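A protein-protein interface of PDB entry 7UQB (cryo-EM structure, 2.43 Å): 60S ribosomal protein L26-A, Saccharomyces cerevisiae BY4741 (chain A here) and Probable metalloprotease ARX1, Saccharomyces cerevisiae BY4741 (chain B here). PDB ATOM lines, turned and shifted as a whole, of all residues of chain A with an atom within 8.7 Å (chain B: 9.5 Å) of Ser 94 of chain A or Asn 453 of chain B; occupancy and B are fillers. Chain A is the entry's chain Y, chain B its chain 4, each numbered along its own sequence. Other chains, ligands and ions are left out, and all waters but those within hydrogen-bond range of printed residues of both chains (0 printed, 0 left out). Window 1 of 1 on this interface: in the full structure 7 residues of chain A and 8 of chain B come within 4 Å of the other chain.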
ATOM      1  N   ASP A  83       9.379  18.735  19.236  1.00  0.00           N
ATOM      2  CA  ASP A  83       7.937  18.959  19.148  1.00  0.00           C
ATOM      3  C   ASP A  83       7.298  18.171  18.006  1.00  0.00           C
ATOM      4  O   ASP A  83       6.198  17.629  18.163  1.00  0.00           O
ATOM      5  CB  ASP A  83       7.652  20.453  18.996  1.00  0.00           C
ATOM      6  CG  ASP A  83       8.521  21.110  17.945  1.00  0.00           C
ATOM      7  OD1 ASP A  83       9.353  20.410  17.332  1.00  0.00           O
ATOM      8  OD2 ASP A  83       8.372  22.332  17.730  1.00  0.00           O
ATOM      9  N   VAL A  85       8.379  15.391  16.466  1.00  0.00           N
ATOM     10  CA  VAL A  85       8.694  13.968  16.423  1.00  0.00           C
ATOM     11  C   VAL A  85       7.883  13.288  17.521  1.00  0.00           C
ATOM     12  O   VAL A  85       8.213  13.384  18.707  1.00  0.00           O
ATOM     13  CB  VAL A  85      10.195  13.719  16.586  1.00  0.00           C
ATOM     14  CG1 VAL A  85      10.498  12.236  16.547  1.00  0.00           C
ATOM     15  CG2 VAL A  85      10.971  14.453  15.505  1.00  0.00           C
ATOM     16  N   THR A  86       6.817  12.590  17.131  1.00  0.00           N
ATOM     17  CA  THR A  86       5.903  11.971  18.080  1.00  0.00           C
ATOM     18  C   THR A  86       5.458  10.609  17.566  1.00  0.00           C
ATOM     19  O   THR A  86       5.617  10.279  16.389  1.00  0.00           O
ATOM     20  CB  THR A  86       4.659  12.839  18.334  1.00  0.00           C
ATOM     21  OG1 THR A  86       4.119  13.280  17.082  1.00  0.00           O
ATOM     22  CG2 THR A  86       4.988  14.045  19.206  1.00  0.00           C
ATOM     23  N   LYS A  87       4.897   9.820  18.476  1.00  0.00           N
ATOM     24  CA  LYS A  87       4.181   8.595  18.150  1.00  0.00           C
ATOM     25  C   LYS A  87       2.702   8.836  18.412  1.00  0.00           C
ATOM     26  O   LYS A  87       2.325   9.277  19.503  1.00  0.00           O
ATOM     27  CB  LYS A  87       4.696   7.417  18.979  1.00  0.00           C
ATOM     28  CG  LYS A  87       4.101   6.068  18.599  1.00  0.00           C
ATOM     29  CD  LYS A  87       4.851   4.930  19.278  1.00  0.00           C
ATOM     30  CE  LYS A  87       4.308   3.571  18.860  1.00  0.00           C
ATOM     31  NZ  LYS A  87       2.895   3.379  19.287  1.00  0.00           N
ATOM     32  N   GLU A  88       1.871   8.564  17.412  1.00  0.00           N
ATOM     33  CA  GLU A  88       0.455   8.892  17.457  1.00  0.00           C
ATOM     34  C   GLU A  88      -0.384   7.627  17.586  1.00  0.00           C
ATOM     35  O   GLU A  88       0.006   6.552  17.124  1.00  0.00           O
ATOM     36  CB  GLU A  88       0.027   9.667  16.204  1.00  0.00           C
ATOM     37  CG  GLU A  88       0.860  10.913  15.906  1.00  0.00           C
ATOM     38  CD  GLU A  88       2.127  10.601  15.127  1.00  0.00           C
ATOM     39  OE1 GLU A  88       2.307   9.432  14.727  1.00  0.00           O
ATOM     40  OE2 GLU A  88       2.944  11.524  14.918  1.00  0.00           O
ATOM     41  N   LYS A  89      -1.539   7.768  18.229  1.00  0.00           N
ATOM     42  CA  LYS A  89      -2.491   6.677  18.379  1.00  0.00           C
ATOM     43  C   LYS A  89      -3.819   7.046  17.727  1.00  0.00           C
ATOM     44  O   LYS A  89      -4.044   8.187  17.318  1.00  0.00           O
ATOM     45  CB  LYS A  89      -2.713   6.330  19.854  1.00  0.00           C
ATOM     46  CG  LYS A  89      -1.454   6.067  20.651  1.00  0.00           C
ATOM     47  CD  LYS A  89      -1.813   5.645  22.061  1.00  0.00           C
ATOM     48  CE  LYS A  89      -0.611   5.618  22.975  1.00  0.00           C
ATOM     49  NZ  LYS A  89      -1.019   5.310  24.369  1.00  0.00           N
ATOM     50  N   VAL A  90      -4.704   6.049  17.637  1.00  0.00           N
ATOM     51  CA  VAL A  90      -6.018   6.260  17.035  1.00  0.00           C
ATOM     52  C   VAL A  90      -6.892   7.132  17.933  1.00  0.00           C
ATOM     53  O   VAL A  90      -7.609   8.017  17.451  1.00  0.00           O
ATOM     54  CB  VAL A  90      -6.677   4.902  16.720  1.00  0.00           C
ATOM     55  CG1 VAL A  90      -8.186   5.039  16.568  1.00  0.00           C
ATOM     56  CG2 VAL A  90      -6.078   4.314  15.451  1.00  0.00           C
ATOM     57  N   ASN A  91      -6.826   6.924  19.249  1.00  0.00           N
ATOM     58  CA  ASN A  91      -7.627   7.717  20.187  1.00  0.00           C
ATOM     59  C   ASN A  91      -7.162   9.179  20.312  1.00  0.00           C
ATOM     60  O   ASN A  91      -7.709   9.890  21.162  1.00  0.00           O
ATOM     61  CB  ASN A  91      -7.634   7.060  21.569  1.00  0.00           C
ATOM     62  CG  ASN A  91      -6.241   6.780  22.098  1.00  0.00           C
ATOM     63  OD1 ASN A  91      -5.247   7.251  21.553  1.00  0.00           O
ATOM     64  ND2 ASN A  91      -6.164   6.005  23.172  1.00  0.00           N
ATOM     65  N   GLY A  92      -6.195   9.647  19.529  1.00  0.00           N
ATOM     66  CA  GLY A  92      -5.738  11.017  19.615  1.00  0.00           C
ATOM     67  C   GLY A  92      -4.549  11.245  20.518  1.00  0.00           C
ATOM     68  O   GLY A  92      -4.185  12.403  20.749  1.00  0.00           O
ATOM     69  N   ALA A  93      -3.935  10.186  21.035  1.00  0.00           N
ATOM     70  CA  ALA A  93      -2.810  10.336  21.942  1.00  0.00           C
ATOM     71  C   ALA A  93      -1.514  10.574  21.176  1.00  0.00           C
ATOM     72  O   ALA A  93      -1.254   9.939  20.149  1.00  0.00           O
ATOM     73  CB  ALA A  93      -2.674   9.103  22.832  1.00  0.00           C
ATOM     74  N   SER A  94      -0.703  11.500  21.684  1.00  0.00           N
ATOM     75  CA  SER A  94       0.618  11.792  21.141  1.00  0.00           C
ATOM     76  C   SER A  94       1.649  11.608  22.244  1.00  0.00           C
ATOM     77  O   SER A  94       1.578  12.278  23.280  1.00  0.00           O
ATOM     78  CB  SER A  94       0.689  13.212  20.579  1.00  0.00           C
ATOM     79  OG  SER A  94      -0.183  13.376  19.478  1.00  0.00           O
ATOM     80  N   VAL A  95       2.600  10.713  22.023  1.00  0.00           N
ATOM     81  CA  VAL A  95       3.683  10.446  22.964  1.00  0.00           C
ATOM     82  C   VAL A  95       4.977  10.956  22.339  1.00  0.00           C
ATOM     83  O   VAL A  95       5.321  10.542  21.227  1.00  0.00           O
ATOM     84  CB  VAL A  95       3.787   8.951  23.303  1.00  0.00           C
ATOM     85  CG1 VAL A  95       4.796   8.731  24.416  1.00  0.00           C
ATOM     86  CG2 VAL A  95       2.426   8.397  23.692  1.00  0.00           C
ATOM     87  N   PRO A  96       5.705  11.859  22.994  1.00  0.00           N
ATOM     88  CA  PRO A  96       6.986  12.314  22.436  1.00  0.00           C
ATOM     89  C   PRO A  96       7.990  11.174  22.338  1.00  0.00           C
ATOM     90  O   PRO A  96       8.032  10.281  23.185  1.00  0.00           O
ATOM     91  CB  PRO A  96       7.449  13.382  23.434  1.00  0.00           C
ATOM     92  CG  PRO A  96       6.219  13.781  24.181  1.00  0.00           C
ATOM     93  CD  PRO A  96       5.368  12.554  24.245  1.00  0.00           C
ATOM     94  N   ILE A  97       8.799  11.212  21.285  1.00  0.00           N
ATOM     95  CA  ILE A  97       9.880  10.251  21.099  1.00  0.00           C
ATOM     96  C   ILE A  97      11.089  10.729  21.889  1.00  0.00           C
ATOM     97  O   ILE A  97      11.474  11.901  21.805  1.00  0.00           O
ATOM     98  CB  ILE A  97      10.222  10.089  19.608  1.00  0.00           C
ATOM     99  CG1 ILE A  97       8.990   9.649  18.816  1.00  0.00           C
ATOM    100  CG2 ILE A  97      11.356   9.092  19.424  1.00  0.00           C
ATOM    101  CD1 ILE A  97       8.466   8.287  19.204  1.00  0.00           C
ATOM    102  N   HIS B 447       0.052  26.260  19.020  1.00  0.00           N
ATOM    103  CA  HIS B 447       0.433  25.697  20.312  1.00  0.00           C
ATOM    104  C   HIS B 447      -0.334  24.411  20.601  1.00  0.00           C
ATOM    105  O   HIS B 447       0.237  23.434  21.104  1.00  0.00           O
ATOM    106  CB  HIS B 447       0.196  26.727  21.415  1.00  0.00           C
ATOM    107  CG  HIS B 447       0.612  26.267  22.776  1.00  0.00           C
ATOM    108  ND1 HIS B 447       1.927  26.030  23.114  1.00  0.00           N
ATOM    109  CD2 HIS B 447      -0.115  26.002  23.887  1.00  0.00           C
ATOM    110  CE1 HIS B 447       1.992  25.639  24.374  1.00  0.00           C
ATOM    111  NE2 HIS B 447       0.767  25.617  24.867  1.00  0.00           N
ATOM    112  N   ILE B 448      -1.630  24.394  20.272  1.00  0.00           N
ATOM    113  CA  ILE B 448      -2.444  23.195  20.443  1.00  0.00           C
ATOM    114  C   ILE B 448      -1.900  22.054  19.595  1.00  0.00           C
ATOM    115  O   ILE B 448      -1.784  20.914  20.062  1.00  0.00           O
ATOM    116  CB  ILE B 448      -3.915  23.499  20.097  1.00  0.00           C
ATOM    117  CG1 ILE B 448      -4.469  24.595  21.010  1.00  0.00           C
ATOM    118  CG2 ILE B 448      -4.764  22.240  20.190  1.00  0.00           C
ATOM    119  CD1 ILE B 448      -5.900  24.984  20.702  1.00  0.00           C
ATOM    120  N   LEU B 449      -1.556  22.343  18.337  1.00  0.00           N
ATOM    121  CA  LEU B 449      -1.040  21.303  17.452  1.00  0.00           C
ATOM    122  C   LEU B 449       0.317  20.787  17.920  1.00  0.00           C
ATOM    123  O   LEU B 449       0.568  19.576  17.891  1.00  0.00           O
ATOM    124  CB  LEU B 449      -0.956  21.827  16.020  1.00  0.00           C
ATOM    125  CG  LEU B 449      -2.298  22.103  15.339  1.00  0.00           C
ATOM    126  CD1 LEU B 449      -2.093  22.645  13.935  1.00  0.00           C
ATOM    127  CD2 LEU B 449      -3.157  20.848  15.313  1.00  0.00           C
ATOM    128  N   LYS B 450       1.202  21.684  18.365  1.00  0.00           N
ATOM    129  CA  LYS B 450       2.519  21.266  18.832  1.00  0.00           C
ATOM    130  C   LYS B 450       2.458  20.515  20.154  1.00  0.00           C
ATOM    131  O   LYS B 450       3.378  19.750  20.459  1.00  0.00           O
ATOM    132  CB  LYS B 450       3.442  22.477  18.984  1.00  0.00           C
ATOM    133  CG  LYS B 450       3.796  23.171  17.684  1.00  0.00           C
ATOM    134  CD  LYS B 450       4.276  24.593  17.950  1.00  0.00           C
ATOM    135  CE  LYS B 450       4.283  25.424  16.677  1.00  0.00           C
ATOM    136  NZ  LYS B 450       4.584  26.858  16.945  1.00  0.00           N
ATOM    137  N   ALA B 451       1.408  20.720  20.943  1.00  0.00           N
ATOM    138  CA  ALA B 451       1.301  20.053  22.230  1.00  0.00           C
ATOM    139  C   ALA B 451       1.086  18.551  22.069  1.00  0.00           C
ATOM    140  O   ALA B 451       0.590  18.075  21.045  1.00  0.00           O
ATOM    141  CB  ALA B 451       0.156  20.650  23.037  1.00  0.00           C
ATOM    142  N   THR B 452       1.471  17.806  23.103  1.00  0.00           N
ATOM    143  CA  THR B 452       1.311  16.359  23.152  1.00  0.00           C
ATOM    144  C   THR B 452       0.371  15.996  24.292  1.00  0.00           C
ATOM    145  O   THR B 452       0.563  16.447  25.426  1.00  0.00           O
ATOM    146  CB  THR B 452       2.657  15.655  23.352  1.00  0.00           C
ATOM    147  OG1 THR B 452       3.286  16.153  24.540  1.00  0.00           O
ATOM    148  CG2 THR B 452       3.571  15.889  22.162  1.00  0.00           C
ATOM    149  N   ASN B 453      -0.638  15.183  23.993  1.00  0.00           N
ATOM    150  CA  ASN B 453      -1.510  14.609  25.017  1.00  0.00           C
ATOM    151  C   ASN B 453      -1.319  13.099  25.032  1.00  0.00           C
ATOM    152  O   ASN B 453      -1.802  12.401  24.126  1.00  0.00           O
ATOM    153  CB  ASN B 453      -2.976  14.974  24.776  1.00  0.00           C
ATOM    154  CG  ASN B 453      -3.374  14.871  23.320  1.00  0.00           C
ATOM    155  OD1 ASN B 453      -2.534  14.964  22.427  1.00  0.00           O
ATOM    156  ND2 ASN B 453      -4.665  14.682  23.073  1.00  0.00           N
ATOM    157  N   PRO B 454      -0.599  12.552  26.018  1.00  0.00           N
ATOM    158  CA  PRO B 454      -0.368  11.098  26.044  1.00  0.00           C
ATOM    159  C   PRO B 454      -1.622  10.267  26.264  1.00  0.00           C
ATOM    160  O   PRO B 454      -1.594   9.062  25.988  1.00  0.00           O
ATOM    161  CB  PRO B 454       0.621  10.922  27.205  1.00  0.00           C
ATOM    162  CG  PRO B 454       1.257  12.266  27.375  1.00  0.00           C
ATOM    163  CD  PRO B 454       0.191  13.257  27.039  1.00  0.00           C
ATOM    164  N   ASN B 455      -2.711  10.855  26.757  1.00  0.00           N
ATOM    165  CA  ASN B 455      -3.921  10.093  27.043  1.00  0.00           C
ATOM    166  C   ASN B 455      -4.923  10.109  25.898  1.00  0.00           C
ATOM    167  O   ASN B 455      -5.691   9.152  25.749  1.00  0.00           O
ATOM    168  CB  ASN B 455      -4.603  10.628  28.305  1.00  0.00           C
ATOM    169  CG  ASN B 455      -3.692  10.607  29.515  1.00  0.00           C
ATOM    170  OD1 ASN B 455      -3.494  11.629  30.173  1.00  0.00           O
ATOM    171  ND2 ASN B 455      -3.134   9.442  29.817  1.00  0.00           N
ATOM    172  N   GLY B 456      -4.937  11.166  25.093  1.00  0.00           N
ATOM    173  CA  GLY B 456      -5.928  11.257  24.031  1.00  0.00           C
ATOM    174  C   GLY B 456      -7.309  11.512  24.602  1.00  0.00           C
ATOM    175  O   GLY B 456      -7.494  12.361  25.481  1.00  0.00           O
ATOM    176  N   ASN B 457      -8.296  10.765  24.101  1.00  0.00           N
ATOM    177  CA  ASN B 457      -9.670  10.900  24.576  1.00  0.00           C
ATOM    178  C   ASN B 457      -9.847  10.436  26.015  1.00  0.00           C
ATOM    179  O   ASN B 457     -10.824  10.830  26.660  1.00  0.00           O
ATOM    180  CB  ASN B 457     -10.622  10.101  23.685  1.00  0.00           C
ATOM    181  CG  ASN B 457     -10.637  10.591  22.258  1.00  0.00           C
ATOM    182  OD1 ASN B 457     -10.468  11.779  21.997  1.00  0.00           O
ATOM    183  ND2 ASN B 457     -10.847   9.672  21.323  1.00  0.00           N
ATOM    184  N   LEU B 458      -8.934   9.607  26.527  1.00  0.00           N
ATOM    185  CA  LEU B 458      -9.168   8.933  27.801  1.00  0.00           C
ATOM    186  C   LEU B 458      -9.135   9.892  28.986  1.00  0.00           C
ATOM    187  O   LEU B 458      -9.765   9.618  30.013  1.00  0.00           O
ATOM    188  CB  LEU B 458      -8.142   7.818  27.998  1.00  0.00           C
ATOM    189  CG  LEU B 458      -8.219   6.644  27.019  1.00  0.00           C
ATOM    190  CD1 LEU B 458      -7.163   5.600  27.348  1.00  0.00           C
ATOM    191  CD2 LEU B 458      -9.607   6.026  27.025  1.00  0.00           C
ATOM    192  N   SER B 459      -8.422  11.010  28.872  1.00  0.00           N
ATOM    193  CA  SER B 459      -8.248  11.894  30.016  1.00  0.00           C
ATOM    194  C   SER B 459      -9.525  12.671  30.318  1.00  0.00           C
ATOM    195  O   SER B 459     -10.271  13.053  29.413  1.00  0.00           O
ATOM    196  CB  SER B 459      -7.091  12.863  29.773  1.00  0.00           C
ATOM    197  OG  SER B 459      -7.319  13.663  28.629  1.00  0.00           O
ATOM    198  N   LEU B 473     -15.381  16.773  25.774  1.00  0.00           N
ATOM    199  CA  LEU B 473     -14.379  16.786  24.708  1.00  0.00           C
ATOM    200  C   LEU B 473     -14.519  18.081  23.919  1.00  0.00           C
ATOM    201  O   LEU B 473     -15.335  18.167  22.989  1.00  0.00           O
ATOM    202  CB  LEU B 473     -14.524  15.574  23.791  1.00  0.00           C
ATOM    203  CG  LEU B 473     -13.662  14.349  24.097  1.00  0.00           C
ATOM    204  CD1 LEU B 473     -13.909  13.257  23.070  1.00  0.00           C
ATOM    205  CD2 LEU B 473     -12.192  14.726  24.132  1.00  0.00           C
ATOM    206  N   LEU B 475     -12.364  19.306  21.826  1.00  0.00           N
ATOM    207  CA  LEU B 475     -11.779  19.090  20.503  1.00  0.00           C
ATOM    208  C   LEU B 475     -11.857  17.604  20.172  1.00  0.00           C
ATOM    209  O   LEU B 475     -10.867  16.873  20.312  1.00  0.00           O
ATOM    210  CB  LEU B 475     -10.339  19.600  20.445  1.00  0.00           C
ATOM    211  CG  LEU B 475     -10.149  21.110  20.610  1.00  0.00           C
ATOM    212  CD1 LEU B 475      -8.674  21.462  20.714  1.00  0.00           C
ATOM    213  CD2 LEU B 475     -10.796  21.856  19.458  1.00  0.00           C
ATOM    214  N   PRO B 476     -13.029  17.122  19.743  1.00  0.00           N
ATOM    215  CA  PRO B 476     -13.175  15.679  19.471  1.00  0.00           C
ATOM    216  C   PRO B 476     -12.289  15.165  18.348  1.00  0.00           C
ATOM    217  O   PRO B 476     -11.792  14.036  18.428  1.00  0.00           O
ATOM    218  CB  PRO B 476     -14.665  15.541  19.120  1.00  0.00           C
ATOM    219  CG  PRO B 476     -15.313  16.789  19.634  1.00  0.00           C
ATOM    220  CD  PRO B 476     -14.280  17.855  19.505  1.00  0.00           C
ATOM    221  N   LYS B 477     -12.078  15.961  17.298  1.00  0.00           N
ATOM    222  CA  LYS B 477     -11.299  15.490  16.159  1.00  0.00           C
ATOM    223  C   LYS B 477      -9.807  15.453  16.458  1.00  0.00           C
ATOM    224  O   LYS B 477      -9.097  14.591  15.931  1.00  0.00           O
ATOM    225  CB  LYS B 477     -11.575  16.367  14.936  1.00  0.00           C
ATOM    226  CG  LYS B 477     -12.998  16.260  14.421  1.00  0.00           C
ATOM    227  CD  LYS B 477     -13.262  17.249  13.300  1.00  0.00           C
ATOM    228  CE  LYS B 477     -14.614  17.000  12.656  1.00  0.00           C
ATOM    229  NZ  LYS B 477     -15.729  17.104  13.636  1.00  0.00           N
ATOM    230  N   LEU B 478      -9.316  16.371  17.288  1.00  0.00           N
ATOM    231  CA  LEU B 478      -7.925  16.366  17.714  1.00  0.00           C
ATOM    232  C   LEU B 478      -7.672  15.464  18.913  1.00  0.00           C
ATOM    233  O   LEU B 478      -6.509  15.258  19.278  1.00  0.00           O
ATOM    234  CB  LEU B 478      -7.468  17.788  18.051  1.00  0.00           C
ATOM    235  CG  LEU B 478      -7.266  18.746  16.880  1.00  0.00           C
ATOM    236  CD1 LEU B 478      -6.964  20.144  17.388  1.00  0.00           C
ATOM    237  CD2 LEU B 478      -6.152  18.247  15.972  1.00  0.00           C
ATOM    238  N   GLY B 479      -8.719  14.920  19.524  1.00  0.00           N
ATOM    239  CA  GLY B 479      -8.565  14.087  20.704  1.00  0.00           C
ATOM    240  C   GLY B 479      -8.052  14.820  21.925  1.00  0.00           C
ATOM    241  O   GLY B 479      -7.178  14.301  22.630  1.00  0.00           O
ATOM    242  N   VAL B 480      -8.574  16.012  22.195  1.00  0.00           N
ATOM    243  CA  VAL B 480      -8.103  16.856  23.288  1.00  0.00           C
ATOM    244  C   VAL B 480      -9.241  17.037  24.281  1.00  0.00           C
ATOM    245  O   VAL B 480     -10.326  17.506  23.914  1.00  0.00           O
ATOM    246  CB  VAL B 480      -7.595  18.214  22.779  1.00  0.00           C
ATOM    247  CG1 VAL B 480      -7.312  19.147  23.944  1.00  0.00           C
ATOM    248  CG2 VAL B 480      -6.349  18.023  21.929  1.00  0.00           C
ATOM    249  N   SER B 481      -8.992  16.678  25.536  1.00  0.00           N
ATOM    250  CA  SER B 481      -9.985  16.803  26.589  1.00  0.00           C
ATOM    251  C   SER B 481      -9.936  18.195  27.218  1.00  0.00           C
ATOM    252  O   SER B 481      -9.058  19.009  26.930  1.00  0.00           O
ATOM    253  CB  SER B 481      -9.774  15.727  27.653  1.00  0.00           C
ATOM    254  OG  SER B 481      -8.505  15.852  28.270  1.00  0.00           O
ATOM    255  N   ALA B 482     -10.911  18.457  28.093  1.00  0.00           N
ATOM    256  CA  ALA B 482     -11.021  19.769  28.725  1.00  0.00           C
ATOM    257  C   ALA B 482      -9.850  20.042  29.661  1.00  0.00           C
ATOM    258  O   ALA B 482      -9.343  21.169  29.713  1.00  0.00           O
ATOM    259  CB  ALA B 482     -12.346  19.877  29.478  1.00  0.00           C
ATOM    260  N   ILE B 483      -9.409  19.028  30.410  1.00  0.00           N
ATOM    261  CA  ILE B 483      -8.266  19.204  31.302  1.00  0.00           C
ATOM    262  C   ILE B 483      -7.003  19.490  30.498  1.00  0.00           C
ATOM    263  O   ILE B 483      -6.199  20.361  30.861  1.00  0.00           O
ATOM    264  CB  ILE B 483      -8.106  17.973  32.220  1.00  0.00           C
ATOM    265  CG1 ILE B 483      -6.801  18.043  33.015  1.00  0.00           C
ATOM    266  CG2 ILE B 483      -8.213  16.672  31.435  1.00  0.00           C
ATOM    267  CD1 ILE B 483      -6.609  16.888  33.977  1.00  0.00           C
ATOM    268  N   LYS B 484      -6.826  18.782  29.379  1.00  0.00           N
ATOM    269  CA  LYS B 484      -5.685  19.032  28.506  1.00  0.00           C
ATOM    270  C   LYS B 484      -5.731  20.438  27.919  1.00  0.00           C
ATOM    271  O   LYS B 484      -4.705  21.121  27.852  1.00  0.00           O
ATOM    272  CB  LYS B 484      -5.640  17.987  27.394  1.00  0.00           C
ATOM    273  CG  LYS B 484      -4.464  18.134  26.449  1.00  0.00           C
ATOM    274  CD  LYS B 484      -3.149  17.988  27.186  1.00  0.00           C
ATOM    275  CE  LYS B 484      -1.979  18.279  26.275  1.00  0.00           C
ATOM    276  NZ  LYS B 484      -0.680  18.127  26.985  1.00  0.00           N
ATOM    277  N   LEU B 485      -6.916  20.893  27.504  1.00  0.00           N
ATOM    278  CA  LEU B 485      -7.029  22.228  26.922  1.00  0.00           C
ATOM    279  C   LEU B 485      -6.773  23.313  27.961  1.00  0.00           C
ATOM    280  O   LEU B 485      -6.147  24.336  27.657  1.00  0.00           O
ATOM    281  CB  LEU B 485      -8.404  22.409  26.279  1.00  0.00           C
ATOM    282  CG  LEU B 485      -8.640  23.740  25.562  1.00  0.00           C
ATOM    283  CD1 LEU B 485      -7.595  23.964  24.476  1.00  0.00           C
ATOM    284  CD2 LEU B 485     -10.043  23.796  24.981  1.00  0.00           C
ATOM    285  N   SER B 487      -4.813  22.930  30.546  1.00  0.00           N
ATOM    286  CA  SER B 487      -3.368  22.877  30.732  1.00  0.00           C
ATOM    287  C   SER B 487      -2.640  23.628  29.624  1.00  0.00           C
ATOM    288  O   SER B 487      -1.664  24.336  29.885  1.00  0.00           O
ATOM    289  CB  SER B 487      -2.902  21.422  30.794  1.00  0.00           C
ATOM    290  OG  SER B 487      -1.512  21.340  31.047  1.00  0.00           O
ATOM    291  N   LEU B 488      -3.106  23.487  28.379  1.00  0.00           N
ATOM    292  CA  LEU B 488      -2.495  24.213  27.267  1.00  0.00           C
ATOM    293  C   LEU B 488      -2.683  25.717  27.413  1.00  0.00           C
ATOM    294  O   LEU B 488      -1.761  26.498  27.139  1.00  0.00           O
ATOM    295  CB  LEU B 488      -3.078  23.739  25.937  1.00  0.00           C
ATOM    296  CG  LEU B 488      -2.817  22.279  25.575  1.00  0.00           C
ATOM    297  CD1 LEU B 488      -3.109  22.018  24.106  1.00  0.00           C
ATOM    298  CD2 LEU B 488      -1.395  21.906  25.942  1.00  0.00           C
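The backbone carbonyl oxygen (O) of Asn 91 of chain A lies within hydrogen-bond range of the backbone NH (N) of Asn 457 of chain B.
The backbone NH (N) of Ser 94 of chain A lies within hydrogen-bond range of the backbone carbonyl oxygen (O) of Asn 453 of chain B, 2.8 Å away.
The backbone carbonyl oxygen (O) of Gly 92 of chain A lies within hydrogen-bond range of the side-chain amide nitrogen (ND2) of Asn 453 of chain B (3.3 Å).
The side-chain amide nitrogen of Asn 453 of chain B lies within hydrogen-bond range of the backbone carbonyl oxygen of Gly 479 of chain B (2.6 Å).
The side-chain amide oxygen of Asn 91 of chain A sits at hydrogen-bond distance from the backbone NH of Ala 93 of chain A.
The side-chain hydroxyl of Ser 459 of chain B sits at hydrogen-bond distance from the backbone carbonyl oxygen of Gly 456 of chain B.
The backbone carbonyl oxygen (O) of Thr 452 of chain B sits at hydrogen-bond distance from the side-chain amino group (NZ) of Lys 484 of chain B (2.6 Å).
OG1 of Thr 86 of chain A is in hydrogen-bond range of OE2 of Glu 88 of chain A.
Among the printed residues, pairs that only touch across the chains: Thr 86 of chain A with Thr 452 of chain B (3.8 Å), Asn 91 of chain A with Gly 456 of chain B (3.6 Å), Gly 92 of chain A with Gly 456 of chain B (3.8 Å), Gly 92 of chain A with Leu 478 of chain B (3.96 Å), Ala 93 of chain A with Asn 453 of chain B (3.2 Å), Ala 93 of chain A with Pro 454 of chain B (3.3 Å), Ala 93 of chain A with Asn 455 of chain B (3.9 Å), Ala 93 of chain A with Gly 456 of chain B (3.8 Å), Ser 94 of chain A with Thr 452 of chain B (3.5 Å), Ser 94 of chain A with Pro 454 of chain B (3.5 Å) and Pro 96 of chain A with Thr 452 of chain B (3.8 Å).
Of chain B, only Thr 452 (3.5 Å), Asn 453 (2.8 Å) and Pro 454 (3.5 Å) come within 4 Å of Ser 94 of chain A.
Asn 453 of chain B touches three residues of chain A.
Ala 93 of chain A touches just these residues of chain B: Asn 453 (3.2 Å), Pro 454 (3.3 Å), Asn 455 (3.9 Å) and Gly 456 (3.8 Å).
No residue of chain B comes within 4 Å of Val 95 of chain A.
Of chain A, only Thr 86 (3.8 Å), Ser 94 (3.5 Å) and Pro 96 (3.8 Å) come within 4 Å of Thr 452 of chain B.
Pro 454 of chain B touches two residues of chain A.
Gly 456 of chain B touches just these residues of chain A: Asn 91, Gly 92 and Ala 93.
Printed residues of chain B within 4 Å of Pro 96 of chain A: Thr 452 (3.8 Å).
Of the printed residues of chain B, Gly 92 of chain A touches Asn 453, Gly 456 and Leu 478.
Of the printed residues of chain A, Asn 455 of chain B touches Ala 93.
Printed residues of chain B within 4 Å of Asn 91 of chain A: Gly 456 and Asn 457.
Lys 87 of chain A touches none of the printed residues of chain B.
The nearest printed residue of chain B that does not touch Thr 86 of chain A is Lys 450 of chain B (6.1 Å).
Of the 14 printed residues of chain A, 6 touch a printed residue of chain B.
Among the printed residues, 14 pairs touch across the chains.
Among the printed residues, no Asp or Glu carboxylate lies within 4 Å of a Lys or Arg side-chain nitrogen of the other chain.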
